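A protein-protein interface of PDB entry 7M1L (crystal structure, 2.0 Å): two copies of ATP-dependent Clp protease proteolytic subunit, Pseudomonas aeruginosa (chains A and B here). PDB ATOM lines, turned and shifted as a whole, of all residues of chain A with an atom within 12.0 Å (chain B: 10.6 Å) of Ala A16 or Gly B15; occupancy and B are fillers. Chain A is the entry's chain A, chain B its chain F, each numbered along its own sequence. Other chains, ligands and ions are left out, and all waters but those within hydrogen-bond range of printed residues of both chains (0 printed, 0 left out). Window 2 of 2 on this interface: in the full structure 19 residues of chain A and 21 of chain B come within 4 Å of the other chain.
NE2 of His A14 is in hydrogen-bond range of OD2 of Asp B44.
NZ of Lys B20 lies within salt-bridge range of OE1 of Glu B23, 3.7 Å away.
Among the printed residues, pairs that only touch across the chains: His A14 with Lys B40 (3.6 Å), Ala A16 with Gly B15 (3.8 Å), Ala A16 with Ala B19 (3.8 Å), Ile A17 with Gly B18 (3.8 Å), Ile A17 with Ala B19 (3.6 Å), Ile A17 with Met B22 (3.6 Å), Ile A17 with Asp B44 (3.9 Å), Leu A21 with Asp B44 (3.5 Å), Leu A21 with Gln B47 (3.7 Å) and Tyr A24 with Glu B23 (3.4 Å).
Gly B15 touches one residue of chain A.
No residue of chain B comes within 4 Å of Gly A15.
Of chain B, only Gly B18, Ala B19, Met B22 and Asp B44 come within 4 Å of Ile A17.
Gly A18 touches none of the printed residues of chain B.
No residue of chain B comes within 4 Å of Ala A19.
No residue of chain A comes within 4 Å of Ala B16.
No residue of chain A comes within 4 Å of Ile B17.
Ala B19 touches just these residues of chain A: Ala A16 (3.8 Å) and Ile A17 (3.6 Å).
Printed residues of chain A within 4 Å of Met B22: Ile A17.
Of the printed residues of chain B, His A14 touches Lys B40 and Asp B44.
Of the printed residues of chain A, Asp B44 touches His A14 (2.7 Å), Ile A17 (3.9 Å) and Leu A21 (3.5 Å).
Of the printed residues of chain B, Leu A21 touches Asp B44 and Gln B47.
Of the printed residues of chain A, Glu B23 touches Tyr A24 (3.4 Å).
Lys B20 touches none of the printed residues of chain A.
The nearest residue of chain B that does not touch Ala A16 is Ala B16 (4.3 Å).
Of the 14 printed residues of chain B, 8 touch a printed residue of chain A.
Hydrophobic or aromatic side chains of chain B that line the printed part of chain A: Ala B19 and Met B22.
Printed residues of chain A that touch a printed residue of chain B: His A14, Ala A16, Ile A17, Leu A21 and Tyr A24.
Among the printed residues, no Asp or Glu carboxylate lies within 4 Å of a Lys or Arg side-chain nitrogen of the other chain.
His A14 touches Asp B44, but with the chains exchanged Asp A44 does not touch His B14 (19.2 Å).
Ala A16 touches Ala B19, but with the chains exchanged Ala A19 does not touch Ala B16 (9.9 Å).
Ile A17 touches Asp B44, but with the chains exchanged Asp A44 does not touch Ile B17 (20.2 Å).
Leu A21 touches Asp B44, but with the chains exchanged Asp A44 does not touch Leu B21 (21.3 Å).
Positions printed for both chains: 14, 15, 16, 17, 18, 19, 20, 21, 22, 23 and 44.
Of the 11 pairs that touch across the chains among the printed residues, none has its exchanged pair printed and touching as well.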
ATOM      1  N   HIS A  14      12.496  -5.137  10.212  1.00  0.00           N
ATOM      2  CA  HIS A  14      11.800  -4.623  11.394  1.00  0.00           C
ATOM      3  C   HIS A  14      12.722  -4.688  12.624  1.00  0.00           C
ATOM      4  O   HIS A  14      12.389  -4.199  13.708  1.00  0.00           O
ATOM      5  CB  HIS A  14      10.511  -5.411  11.642  1.00  0.00           C
ATOM      6  CG  HIS A  14       9.676  -4.865  12.759  1.00  0.00           C
ATOM      7  ND1 HIS A  14       9.716  -5.374  14.039  1.00  0.00           N
ATOM      8  CD2 HIS A  14       8.769  -3.858  12.782  1.00  0.00           C
ATOM      9  CE1 HIS A  14       8.878  -4.697  14.805  1.00  0.00           C
ATOM     10  NE2 HIS A  14       8.289  -3.773  14.065  1.00  0.00           N
ATOM     11  N   GLY A  15      13.887  -5.312  12.445  1.00  0.00           N
ATOM     12  CA  GLY A  15      14.855  -5.369  13.525  1.00  0.00           C
ATOM     13  C   GLY A  15      15.277  -3.992  13.999  1.00  0.00           C
ATOM     14  O   GLY A  15      15.406  -3.753  15.202  1.00  0.00           O
ATOM     15  N   ALA A  16      15.482  -3.062  13.063  1.00  0.00           N
ATOM     16  CA  ALA A  16      15.913  -1.721  13.447  1.00  0.00           C
ATOM     17  C   ALA A  16      14.844  -1.018  14.278  1.00  0.00           C
ATOM     18  O   ALA A  16      15.153  -0.363  15.280  1.00  0.00           O
ATOM     19  CB  ALA A  16      16.247  -0.904  12.204  1.00  0.00           C
ATOM     20  N   ILE A  17      13.580  -1.172  13.906  1.00  0.00           N
ATOM     21  CA  ILE A  17      12.515  -0.557  14.692  1.00  0.00           C
ATOM     22  C   ILE A  17      12.457  -1.191  16.075  1.00  0.00           C
ATOM     23  O   ILE A  17      12.398  -0.496  17.095  1.00  0.00           O
ATOM     24  CB  ILE A  17      11.168  -0.670  13.959  1.00  0.00           C
ATOM     25  CG1 ILE A  17      11.171   0.264  12.755  1.00  0.00           C
ATOM     26  CG2 ILE A  17      10.042  -0.315  14.899  1.00  0.00           C
ATOM     27  CD1 ILE A  17       9.927   0.201  11.940  1.00  0.00           C
ATOM     28  N   GLY A  18      12.467  -2.524  16.123  1.00  0.00           N
ATOM     29  CA  GLY A  18      12.440  -3.205  17.407  1.00  0.00           C
ATOM     30  C   GLY A  18      13.618  -2.827  18.280  1.00  0.00           C
ATOM     31  O   GLY A  18      13.474  -2.647  19.486  1.00  0.00           O
ATOM     32  N   ALA A  19      14.798  -2.670  17.676  1.00  0.00           N
ATOM     33  CA  ALA A  19      15.973  -2.302  18.458  1.00  0.00           C
ATOM     34  C   ALA A  19      15.830  -0.911  19.070  1.00  0.00           C
ATOM     35  O   ALA A  19      16.253  -0.685  20.210  1.00  0.00           O
ATOM     36  CB  ALA A  19      17.226  -2.377  17.585  1.00  0.00           C
ATOM     37  N   LYS A  20      15.298   0.052  18.313  1.00  0.00           N
ATOM     38  CA  LYS A  20      15.095   1.392  18.859  1.00  0.00           C
ATOM     39  C   LYS A  20      14.000   1.404  19.932  1.00  0.00           C
ATOM     40  O   LYS A  20      14.155   2.063  20.964  1.00  0.00           O
ATOM     41  CB  LYS A  20      14.806   2.393  17.734  1.00  0.00           C
ATOM     42  CG  LYS A  20      14.867   3.854  18.208  1.00  0.00           C
ATOM     43  CD  LYS A  20      16.162   4.265  18.945  1.00  0.00           C
ATOM     44  CE  LYS A  20      17.454   4.185  18.157  1.00  0.00           C
ATOM     45  NZ  LYS A  20      18.611   4.711  18.984  1.00  0.00           N
ATOM     46  N   LEU A  21      12.895   0.689  19.717  1.00  0.00           N
ATOM     47  CA  LEU A  21      11.868   0.625  20.765  1.00  0.00           C
ATOM     48  C   LEU A  21      12.420  -0.051  22.012  1.00  0.00           C
ATOM     49  O   LEU A  21      12.114   0.357  23.140  1.00  0.00           O
ATOM     50  CB  LEU A  21      10.621  -0.104  20.272  1.00  0.00           C
ATOM     51  CG  LEU A  21       9.831   0.641  19.194  1.00  0.00           C
ATOM     52  CD1 LEU A  21       8.664  -0.210  18.698  1.00  0.00           C
ATOM     53  CD2 LEU A  21       9.345   1.989  19.691  1.00  0.00           C
ATOM     54  N   MET A  22      13.242  -1.085  21.818  1.00  0.00           N
ATOM     55  CA  MET A  22      13.980  -1.720  22.914  1.00  0.00           C
ATOM     56  C   MET A  22      14.759  -0.704  23.731  1.00  0.00           C
ATOM     57  O   MET A  22      14.666  -0.665  24.962  1.00  0.00           O
ATOM     58  CB  MET A  22      14.958  -2.728  22.304  1.00  0.00           C
ATOM     59  CG  MET A  22      15.986  -3.380  23.231  1.00  0.00           C
ATOM     60  SD  MET A  22      15.258  -4.319  24.528  1.00  0.00           S
ATOM     61  CE  MET A  22      14.747  -5.742  23.567  1.00  0.00           C
ATOM     62  N   GLU A  23      15.554   0.115  23.048  1.00  0.00           N
ATOM     63  CA  GLU A  23      16.391   1.097  23.722  1.00  0.00           C
ATOM     64  C   GLU A  23      15.557   2.064  24.556  1.00  0.00           C
ATOM     65  O   GLU A  23      15.905   2.358  25.707  1.00  0.00           O
ATOM     66  CB  GLU A  23      17.224   1.849  22.679  1.00  0.00           C
ATOM     67  CG  GLU A  23      18.089   2.940  23.247  1.00  0.00           C
ATOM     68  CD  GLU A  23      18.871   3.697  22.178  1.00  0.00           C
ATOM     69  OE1 GLU A  23      19.149   3.126  21.097  1.00  0.00           O
ATOM     70  OE2 GLU A  23      19.205   4.873  22.426  1.00  0.00           O
ATOM     71  N   TYR A  24      14.471   2.600  23.979  1.00  0.00           N
ATOM     72  CA  TYR A  24      13.632   3.547  24.718  1.00  0.00           C
ATOM     73  C   TYR A  24      12.940   2.881  25.896  1.00  0.00           C
ATOM     74  O   TYR A  24      12.779   3.500  26.950  1.00  0.00           O
ATOM     75  CB  TYR A  24      12.566   4.191  23.822  1.00  0.00           C
ATOM     76  CG  TYR A  24      13.062   5.260  22.892  1.00  0.00           C
ATOM     77  CD1 TYR A  24      13.025   6.605  23.266  1.00  0.00           C
ATOM     78  CD2 TYR A  24      13.535   4.944  21.641  1.00  0.00           C
ATOM     79  CE1 TYR A  24      13.478   7.603  22.413  1.00  0.00           C
ATOM     80  CE2 TYR A  24      14.012   5.934  20.780  1.00  0.00           C
ATOM     81  CZ  TYR A  24      13.979   7.257  21.171  1.00  0.00           C
ATOM     82  OH  TYR A  24      14.440   8.232  20.303  1.00  0.00           O
ATOM     83  N   ALA A  25      12.465   1.649  25.708  1.00  0.00           N
ATOM     84  CA  ALA A  25      11.775   0.940  26.785  1.00  0.00           C
ATOM     85  C   ALA A  25      12.709   0.703  27.967  1.00  0.00           C
ATOM     86  O   ALA A  25      12.306   0.839  29.130  1.00  0.00           O
ATOM     87  CB  ALA A  25      11.210  -0.382  26.264  1.00  0.00           C
ATOM     88  N   ASP A  44      16.592 -12.294  25.612  1.00  0.00           N
ATOM     89  CA  ASP A  44      16.437 -10.840  25.614  1.00  0.00           C
ATOM     90  C   ASP A  44      15.900 -10.328  26.947  1.00  0.00           C
ATOM     91  O   ASP A  44      16.383  -9.318  27.478  1.00  0.00           O
ATOM     92  CB  ASP A  44      15.498 -10.403  24.487  1.00  0.00           C
ATOM     93  CG  ASP A  44      16.077 -10.640  23.105  1.00  0.00           C
ATOM     94  OD1 ASP A  44      17.294 -10.909  22.979  1.00  0.00           O
ATOM     95  OD2 ASP A  44      15.290 -10.582  22.140  1.00  0.00           O
ATOM     96  N   HIS B  14      13.959  -1.189   4.244  1.00  0.00           N
ATOM     97  CA  HIS B  14      13.067  -0.148   4.751  1.00  0.00           C
ATOM     98  C   HIS B  14      13.109  -0.050   6.269  1.00  0.00           C
ATOM     99  O   HIS B  14      12.509   0.852   6.861  1.00  0.00           O
ATOM    100  CB  HIS B  14      11.622  -0.409   4.302  1.00  0.00           C
ATOM    101  CG  HIS B  14      10.648   0.634   4.763  1.00  0.00           C
ATOM    102  ND1 HIS B  14       9.868   0.479   5.891  1.00  0.00           N
ATOM    103  CD2 HIS B  14      10.325   1.842   4.247  1.00  0.00           C
ATOM    104  CE1 HIS B  14       9.113   1.550   6.056  1.00  0.00           C
ATOM    105  NE2 HIS B  14       9.372   2.394   5.071  1.00  0.00           N
ATOM    106  N   GLY B  15      13.804  -0.992   6.908  1.00  0.00           N
ATOM    107  CA  GLY B  15      13.896  -0.948   8.357  1.00  0.00           C
ATOM    108  C   GLY B  15      14.528   0.330   8.866  1.00  0.00           C
ATOM    109  O   GLY B  15      13.991   0.979   9.764  1.00  0.00           O
ATOM    110  N   ALA B  16      15.626   0.757   8.240  1.00  0.00           N
ATOM    111  CA  ALA B  16      16.322   1.958   8.690  1.00  0.00           C
ATOM    112  C   ALA B  16      15.442   3.194   8.524  1.00  0.00           C
ATOM    113  O   ALA B  16      15.417   4.067   9.398  1.00  0.00           O
ATOM    114  CB  ALA B  16      17.641   2.107   7.931  1.00  0.00           C
ATOM    115  N   ILE B  17      14.679   3.272   7.431  1.00  0.00           N
ATOM    116  CA  ILE B  17      13.786   4.420   7.251  1.00  0.00           C
ATOM    117  C   ILE B  17      12.711   4.426   8.329  1.00  0.00           C
ATOM    118  O   ILE B  17      12.498   5.428   9.026  1.00  0.00           O
ATOM    119  CB  ILE B  17      13.163   4.403   5.838  1.00  0.00           C
ATOM    120  CG1 ILE B  17      14.202   4.770   4.782  1.00  0.00           C
ATOM    121  CG2 ILE B  17      11.972   5.345   5.796  1.00  0.00           C
ATOM    122  CD1 ILE B  17      13.706   4.729   3.334  1.00  0.00           C
ATOM    123  N   GLY B  18      12.023   3.300   8.497  1.00  0.00           N
ATOM    124  CA  GLY B  18      10.972   3.245   9.497  1.00  0.00           C
ATOM    125  C   GLY B  18      11.482   3.555  10.892  1.00  0.00           C
ATOM    126  O   GLY B  18      10.801   4.213  11.682  1.00  0.00           O
ATOM    127  N   ALA B  19      12.687   3.089  11.215  1.00  0.00           N
ATOM    128  CA  ALA B  19      13.238   3.360  12.542  1.00  0.00           C
ATOM    129  C   ALA B  19      13.546   4.844  12.731  1.00  0.00           C
ATOM    130  O   ALA B  19      13.264   5.409  13.797  1.00  0.00           O
ATOM    131  CB  ALA B  19      14.488   2.509  12.778  1.00  0.00           C
ATOM    132  N   LYS B  20      14.118   5.503  11.709  1.00  0.00           N
ATOM    133  CA  LYS B  20      14.392   6.930  11.854  1.00  0.00           C
ATOM    134  C   LYS B  20      13.087   7.731  11.985  1.00  0.00           C
ATOM    135  O   LYS B  20      12.990   8.647  12.808  1.00  0.00           O
ATOM    136  CB  LYS B  20      15.214   7.453  10.673  1.00  0.00           C
ATOM    137  CG  LYS B  20      15.911   8.767  11.006  1.00  0.00           C
ATOM    138  CD  LYS B  20      16.845   8.538  12.213  1.00  0.00           C
ATOM    139  CE  LYS B  20      17.770   9.705  12.512  1.00  0.00           C
ATOM    140  NZ  LYS B  20      18.680   9.371  13.652  1.00  0.00           N
ATOM    141  N   LEU B  21      12.070   7.401  11.187  1.00  0.00           N
ATOM    142  CA  LEU B  21      10.789   8.093  11.315  1.00  0.00           C
ATOM    143  C   LEU B  21      10.130   7.806  12.669  1.00  0.00           C
ATOM    144  O   LEU B  21       9.528   8.699  13.275  1.00  0.00           O
ATOM    145  CB  LEU B  21       9.867   7.695  10.163  1.00  0.00           C
ATOM    146  CG  LEU B  21      10.319   8.146   8.767  1.00  0.00           C
ATOM    147  CD1 LEU B  21       9.321   7.634   7.711  1.00  0.00           C
ATOM    148  CD2 LEU B  21      10.470   9.641   8.692  1.00  0.00           C
ATOM    149  N   MET B  22      10.227   6.564  13.153  1.00  0.00           N
ATOM    150  CA  MET B  22       9.748   6.234  14.499  1.00  0.00           C
ATOM    151  C   MET B  22      10.358   7.163  15.544  1.00  0.00           C
ATOM    152  O   MET B  22       9.661   7.708  16.404  1.00  0.00           O
ATOM    153  CB  MET B  22      10.098   4.777  14.820  1.00  0.00           C
ATOM    154  CG  MET B  22       9.750   4.295  16.234  1.00  0.00           C
ATOM    155  SD  MET B  22       8.008   3.956  16.447  1.00  0.00           S
ATOM    156  CE  MET B  22       7.823   2.512  15.398  1.00  0.00           C
ATOM    157  N   GLU B  23      11.672   7.335  15.496  1.00  0.00           N
ATOM    158  CA  GLU B  23      12.340   8.202  16.453  1.00  0.00           C
ATOM    159  C   GLU B  23      11.795   9.620  16.384  1.00  0.00           C
ATOM    160  O   GLU B  23      11.504  10.235  17.414  1.00  0.00           O
ATOM    161  CB  GLU B  23      13.839   8.162  16.193  1.00  0.00           C
ATOM    162  CG  GLU B  23      14.650   9.068  17.052  1.00  0.00           C
ATOM    163  CD  GLU B  23      16.125   8.969  16.719  1.00  0.00           C
ATOM    164  OE1 GLU B  23      16.550   7.896  16.229  1.00  0.00           O
ATOM    165  OE2 GLU B  23      16.841   9.971  16.920  1.00  0.00           O
ATOM    166  N   LEU B  26       8.123   9.755  17.717  1.00  0.00           N
ATOM    167  CA  LEU B  26       8.099   9.752  19.174  1.00  0.00           C
ATOM    168  C   LEU B  26       8.403  11.136  19.733  1.00  0.00           C
ATOM    169  O   LEU B  26       7.735  11.601  20.667  1.00  0.00           O
ATOM    170  CB  LEU B  26       9.115   8.736  19.694  1.00  0.00           C
ATOM    171  CG  LEU B  26       8.688   7.274  19.765  1.00  0.00           C
ATOM    172  CD1 LEU B  26       9.876   6.408  20.222  1.00  0.00           C
ATOM    173  CD2 LEU B  26       7.503   7.104  20.690  1.00  0.00           C
ATOM    174  N   LYS B  40       2.335  -7.288  14.688  1.00  0.00           N
ATOM    175  CA  LYS B  40       3.521  -6.440  14.632  1.00  0.00           C
ATOM    176  C   LYS B  40       3.159  -4.976  14.883  1.00  0.00           C
ATOM    177  O   LYS B  40       3.865  -4.266  15.611  1.00  0.00           O
ATOM    178  CB  LYS B  40       4.228  -6.624  13.284  1.00  0.00           C
ATOM    179  CG  LYS B  40       5.355  -5.643  13.029  1.00  0.00           C
ATOM    180  CD  LYS B  40       6.035  -5.869  11.664  1.00  0.00           C
ATOM    181  CE  LYS B  40       5.178  -5.340  10.514  1.00  0.00           C
ATOM    182  NZ  LYS B  40       5.080  -3.843  10.565  1.00  0.00           N
ATOM    183  N   ASP B  44       4.390  -2.647  18.262  1.00  0.00           N
ATOM    184  CA  ASP B  44       5.062  -1.357  18.129  1.00  0.00           C
ATOM    185  C   ASP B  44       4.245  -0.236  18.759  1.00  0.00           C
ATOM    186  O   ASP B  44       4.792   0.635  19.449  1.00  0.00           O
ATOM    187  CB  ASP B  44       5.312  -1.025  16.655  1.00  0.00           C
ATOM    188  CG  ASP B  44       6.352  -1.922  16.004  1.00  0.00           C
ATOM    189  OD1 ASP B  44       7.053  -2.670  16.731  1.00  0.00           O
ATOM    190  OD2 ASP B  44       6.477  -1.849  14.754  1.00  0.00           O
ATOM    191  N   GLN B  47       4.219  -0.243  22.669  1.00  0.00           N
ATOM    192  CA  GLN B  47       5.468   0.265  23.222  1.00  0.00           C
ATOM    193  C   GLN B  47       5.597   1.778  23.063  1.00  0.00           C
ATOM    194  O   GLN B  47       6.013   2.482  23.999  1.00  0.00           O
ATOM    195  CB  GLN B  47       6.625  -0.472  22.555  1.00  0.00           C
ATOM    196  CG  GLN B  47       6.763  -1.938  22.964  1.00  0.00           C
ATOM    197  CD  GLN B  47       8.017  -2.544  22.358  1.00  0.00           C
ATOM    198  OE1 GLN B  47       9.107  -2.294  22.838  1.00  0.00           O
ATOM    199  NE2 GLN B  47       7.859  -3.386  21.342  1.00  0.00           N
